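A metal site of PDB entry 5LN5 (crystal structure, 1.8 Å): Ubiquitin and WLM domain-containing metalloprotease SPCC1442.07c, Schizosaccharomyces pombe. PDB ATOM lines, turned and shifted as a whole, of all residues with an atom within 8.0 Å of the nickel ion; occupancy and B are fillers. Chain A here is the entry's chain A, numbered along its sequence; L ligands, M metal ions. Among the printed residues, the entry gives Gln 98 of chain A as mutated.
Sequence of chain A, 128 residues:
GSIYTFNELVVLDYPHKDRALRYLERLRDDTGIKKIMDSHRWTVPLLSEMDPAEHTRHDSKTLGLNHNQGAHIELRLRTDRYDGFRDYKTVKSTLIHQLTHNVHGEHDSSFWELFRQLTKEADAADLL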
ATOM      1  N   THR A  62     -26.229   9.182 -13.378  1.00  0.00           N
ATOM      2  CA  THR A  62     -25.334   8.169 -12.818  1.00  0.00           C
ATOM      3  C   THR A  62     -24.160   8.831 -12.088  1.00  0.00           C
ATOM      4  O   THR A  62     -23.319   9.469 -12.712  1.00  0.00           O
ATOM      5  CB  THR A  62     -24.805   7.231 -13.930  1.00  0.00           C
ATOM      6  OG1 THR A  62     -25.901   6.731 -14.699  1.00  0.00           O
ATOM      7  CG2 THR A  62     -24.035   6.061 -13.331  1.00  0.00           C
ATOM      8  N   GLY A  64     -22.253   6.996  -9.782  1.00  0.00           N
ATOM      9  CA  GLY A  64     -21.312   5.942  -9.436  1.00  0.00           C
ATOM     10  C   GLY A  64     -21.602   4.629 -10.125  1.00  0.00           C
ATOM     11  O   GLY A  64     -22.710   4.423 -10.621  1.00  0.00           O
ATOM     12  N   LEU A  65     -20.604   3.757 -10.149  1.00  0.00           N
ATOM     13  CA  LEU A  65     -20.747   2.407 -10.705  1.00  0.00           C
ATOM     14  C   LEU A  65     -20.056   1.396  -9.819  1.00  0.00           C
ATOM     15  O   LEU A  65     -19.053   1.708  -9.177  1.00  0.00           O
ATOM     16  CB  LEU A  65     -20.121   2.318 -12.098  1.00  0.00           C
ATOM     17  CG  LEU A  65     -20.690   3.220 -13.185  1.00  0.00           C
ATOM     18  CD1 LEU A  65     -19.767   3.192 -14.394  1.00  0.00           C
ATOM     19  CD2 LEU A  65     -22.102   2.781 -13.547  1.00  0.00           C
ATOM     20  N   ASN A  66     -20.583   0.178  -9.823  1.00  0.00           N
ATOM     21  CA  ASN A  66     -19.952  -0.948  -9.156  1.00  0.00           C
ATOM     22  C   ASN A  66     -19.703  -2.036 -10.191  1.00  0.00           C
ATOM     23  O   ASN A  66     -20.654  -2.624 -10.728  1.00  0.00           O
ATOM     24  CB  ASN A  66     -20.832  -1.455  -8.015  1.00  0.00           C
ATOM     25  CG  ASN A  66     -20.205  -2.641  -7.290  1.00  0.00           C
ATOM     26  OD1 ASN A  66     -19.571  -3.495  -7.897  1.00  0.00           O
ATOM     27  ND2 ASN A  66     -20.420  -2.703  -5.978  1.00  0.00           N
ATOM     28  N   THR A  94     -23.921   7.908  -2.388  1.00  0.00           N
ATOM     29  CA  THR A  94     -23.667   7.216  -3.648  1.00  0.00           C
ATOM     30  C   THR A  94     -22.706   6.039  -3.460  1.00  0.00           C
ATOM     31  O   THR A  94     -22.891   4.983  -4.053  1.00  0.00           O
ATOM     32  CB  THR A  94     -23.113   8.188  -4.712  1.00  0.00           C
ATOM     33  OG1 THR A  94     -24.108   9.181  -5.012  1.00  0.00           O
ATOM     34  CG2 THR A  94     -22.725   7.463  -5.989  1.00  0.00           C
ATOM     35  N   HIS A  97     -24.667   3.378  -1.806  1.00  0.00           N
ATOM     36  CA  HIS A  97     -25.422   2.835  -2.922  1.00  0.00           C
ATOM     37  C   HIS A  97     -24.611   1.785  -3.674  1.00  0.00           C
ATOM     38  O   HIS A  97     -25.076   0.656  -3.873  1.00  0.00           O
ATOM     39  CB  HIS A  97     -25.825   3.978  -3.855  1.00  0.00           C
ATOM     40  CG  HIS A  97     -26.654   3.558  -5.017  1.00  0.00           C
ATOM     41  ND1 HIS A  97     -27.886   4.108  -5.290  1.00  0.00           N
ATOM     42  CD2 HIS A  97     -26.424   2.643  -5.991  1.00  0.00           C
ATOM     43  CE1 HIS A  97     -28.385   3.551  -6.376  1.00  0.00           C
ATOM     44  NE2 HIS A  97     -27.518   2.664  -6.819  1.00  0.00           N
ATOM     45  N   GLN A  98     -23.400   2.148  -4.090  1.00  0.00           N
ATOM     46  CA  GLN A  98     -22.527   1.221  -4.824  1.00  0.00           C
ATOM     47  C   GLN A  98     -22.172  -0.007  -3.983  1.00  0.00           C
ATOM     48  O   GLN A  98     -22.117  -1.124  -4.511  1.00  0.00           O
ATOM     49  CB  GLN A  98     -21.228   1.894  -5.291  1.00  0.00           C
ATOM     50  CG  GLN A  98     -21.396   3.115  -6.185  1.00  0.00           C
ATOM     51  CD  GLN A  98     -22.593   3.028  -7.109  1.00  0.00           C
ATOM     52  OE1 GLN A  98     -23.420   3.942  -7.158  1.00  0.00           O
ATOM     53  NE2 GLN A  98     -22.696   1.929  -7.856  1.00  0.00           N
ATOM     54  N   THR A 100     -24.058  -1.232  -1.630  1.00  0.00           N
ATOM     55  CA  THR A 100     -25.309  -2.018  -1.612  1.00  0.00           C
ATOM     56  C   THR A 100     -25.396  -2.948  -2.822  1.00  0.00           C
ATOM     57  O   THR A 100     -25.936  -4.046  -2.727  1.00  0.00           O
ATOM     58  CB  THR A 100     -26.565  -1.116  -1.572  1.00  0.00           C
ATOM     59  OG1 THR A 100     -26.428  -0.152  -0.529  1.00  0.00           O
ATOM     60  CG2 THR A 100     -27.839  -1.938  -1.332  1.00  0.00           C
ATOM     61  N   HIS A 101     -24.862  -2.492  -3.965  1.00  0.00           N
ATOM     62  CA  HIS A 101     -24.788  -3.326  -5.168  1.00  0.00           C
ATOM     63  C   HIS A 101     -23.865  -4.531  -5.054  1.00  0.00           C
ATOM     64  O   HIS A 101     -23.894  -5.388  -5.927  1.00  0.00           O
ATOM     65  CB  HIS A 101     -24.362  -2.510  -6.402  1.00  0.00           C
ATOM     66  CG  HIS A 101     -25.493  -1.784  -7.062  1.00  0.00           C
ATOM     67  ND1 HIS A 101     -26.736  -2.357  -7.258  1.00  0.00           N
ATOM     68  CD2 HIS A 101     -25.549  -0.552  -7.611  1.00  0.00           C
ATOM     69  CE1 HIS A 101     -27.513  -1.486  -7.877  1.00  0.00           C
ATOM     70  NE2 HIS A 101     -26.814  -0.386  -8.104  1.00  0.00           N
ATOM     71  N   HIS A 104     -27.163  -6.643  -3.991  1.00  0.00           N
ATOM     72  CA  HIS A 104     -28.323  -6.571  -4.872  1.00  0.00           C
ATOM     73  C   HIS A 104     -27.998  -5.743  -6.111  1.00  0.00           C
ATOM     74  O   HIS A 104     -27.796  -4.542  -6.021  1.00  0.00           O
ATOM     75  CB  HIS A 104     -29.518  -5.956  -4.138  1.00  0.00           C
ATOM     76  CG  HIS A 104     -29.943  -6.738  -2.930  1.00  0.00           C
ATOM     77  ND1 HIS A 104     -29.876  -6.216  -1.660  1.00  0.00           N
ATOM     78  CD2 HIS A 104     -30.435  -7.989  -2.802  1.00  0.00           C
ATOM     79  CE1 HIS A 104     -30.309  -7.113  -0.794  1.00  0.00           C
ATOM     80  NE2 HIS A 104     -30.653  -8.206  -1.467  1.00  0.00           N
ATOM     81  N   GLY A 105     -27.969  -6.405  -7.267  1.00  0.00           N
ATOM     82  CA  GLY A 105     -27.638  -5.749  -8.542  1.00  0.00           C
ATOM     83  C   GLY A 105     -28.721  -4.830  -9.076  1.00  0.00           C
ATOM     84  O   GLY A 105     -28.418  -3.815  -9.705  1.00  0.00           O
ATOM     85  N   GLU A 106     -29.980  -5.191  -8.828  1.00  0.00           N
ATOM     86  CA  GLU A 106     -31.137  -4.440  -9.311  1.00  0.00           C
ATOM     87  C   GLU A 106     -31.695  -3.606  -8.153  1.00  0.00           C
ATOM     88  O   GLU A 106     -31.581  -3.997  -7.003  1.00  0.00           O
ATOM     89  CB  GLU A 106     -32.206  -5.419  -9.818  1.00  0.00           C
ATOM     90  CG  GLU A 106     -32.839  -5.052 -11.159  1.00  0.00           C
ATOM     91  CD  GLU A 106     -33.769  -6.142 -11.683  1.00  0.00           C
ATOM     92  OE1 GLU A 106     -34.237  -6.973 -10.886  1.00  0.00           O
ATOM     93  OE2 GLU A 106     -34.017  -6.155 -12.898  1.00  0.00           O
ATOM     94  N   HIS A 107     -32.306  -2.464  -8.468  1.00  0.00           N
ATOM     95  CA  HIS A 107     -32.879  -1.589  -7.439  1.00  0.00           C
ATOM     96  C   HIS A 107     -34.278  -2.055  -7.019  1.00  0.00           C
ATOM     97  O   HIS A 107     -35.257  -1.313  -7.147  1.00  0.00           O
ATOM     98  CB  HIS A 107     -32.945  -0.140  -7.925  1.00  0.00           C
ATOM     99  CG  HIS A 107     -31.628   0.392  -8.391  1.00  0.00           C
ATOM    100  ND1 HIS A 107     -31.225   0.310  -9.701  1.00  0.00           N
ATOM    101  CD2 HIS A 107     -30.625   1.004  -7.716  1.00  0.00           C
ATOM    102  CE1 HIS A 107     -30.021   0.854  -9.820  1.00  0.00           C
ATOM    103  NE2 HIS A 107     -29.646   1.286  -8.633  1.00  0.00           N
ATOM    104  N   PHE A 111     -32.856  -4.367  -2.379  1.00  0.00           N
ATOM    105  CA  PHE A 111     -31.815  -3.344  -2.496  1.00  0.00           C
ATOM    106  C   PHE A 111     -32.099  -2.185  -1.555  1.00  0.00           C
ATOM    107  O   PHE A 111     -31.215  -1.741  -0.805  1.00  0.00           O
ATOM    108  CB  PHE A 111     -31.718  -2.818  -3.934  1.00  0.00           C
ATOM    109  CG  PHE A 111     -30.817  -1.616  -4.085  1.00  0.00           C
ATOM    110  CD1 PHE A 111     -29.496  -1.774  -4.482  1.00  0.00           C
ATOM    111  CD2 PHE A 111     -31.284  -0.329  -3.846  1.00  0.00           C
ATOM    112  CE1 PHE A 111     -28.653  -0.679  -4.617  1.00  0.00           C
ATOM    113  CE2 PHE A 111     -30.453   0.773  -3.980  1.00  0.00           C
ATOM    114  CZ  PHE A 111     -29.136   0.594  -4.369  1.00  0.00           C
ATOM    115  N   TRP A 112     -33.332  -1.678  -1.602  1.00  0.00           N
ATOM    116  CA  TRP A 112     -33.713  -0.522  -0.799  1.00  0.00           C
ATOM    117  C   TRP A 112     -33.702  -0.851   0.693  1.00  0.00           C
ATOM    118  O   TRP A 112     -33.360   0.010   1.505  1.00  0.00           O
ATOM    119  CB  TRP A 112     -35.052   0.041  -1.257  1.00  0.00           C
ATOM    120  CG  TRP A 112     -34.936   0.782  -2.561  1.00  0.00           C
ATOM    121  CD1 TRP A 112     -35.475   0.423  -3.765  1.00  0.00           C
ATOM    122  CD2 TRP A 112     -34.212   1.988  -2.804  1.00  0.00           C
ATOM    123  NE1 TRP A 112     -35.135   1.333  -4.737  1.00  0.00           N
ATOM    124  CE2 TRP A 112     -34.357   2.301  -4.166  1.00  0.00           C
ATOM    125  CE3 TRP A 112     -33.441   2.831  -1.991  1.00  0.00           C
ATOM    126  CZ2 TRP A 112     -33.772   3.433  -4.743  1.00  0.00           C
ATOM    127  CZ3 TRP A 112     -32.859   3.956  -2.560  1.00  0.00           C
ATOM    128  CH2 TRP A 112     -33.025   4.247  -3.924  1.00  0.00           C
HETATM  129  C1  LIG L   1     -26.340   2.183 -10.643  1.00  0.00           C
HETATM  130  O1  LIG L   1     -27.041   3.170 -10.813  1.00  0.00           O
HETATM  131  O2  LIG L   1     -25.244   2.292 -10.116  1.00  0.00           O
HETATM  132  O3  LIG L   1     -26.755   1.081 -10.985  1.00  0.00           O
HETATM  133 NI    NI M   1     -27.413   1.592  -8.752  1.00  0.00          NI
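ND1 of His 101 sits close to O of Gly 105 (3.3 Å). A ring nitrogen (ND1) of His 101 lies within hydrogen-bond range of the backbone carbonyl oxygen (O) of His 104 (2.7 Å).
The nearest printed residue that does not touch the nickel ion is Gln 98 (4.8 Å).
The nickel ion is bound by a ring nitrogen (NE2) of His 101, a ring nitrogen (NE2) of His 97, a ring nitrogen (NE2) of His 107 and an oxygen (O3) of the ligand. Slightly farther from the nickel ion lies O1 of the ligand (2.6 Å). Slightly farther from the nickel ion lies an oxygen (O2) of the ligand (2.7 Å).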
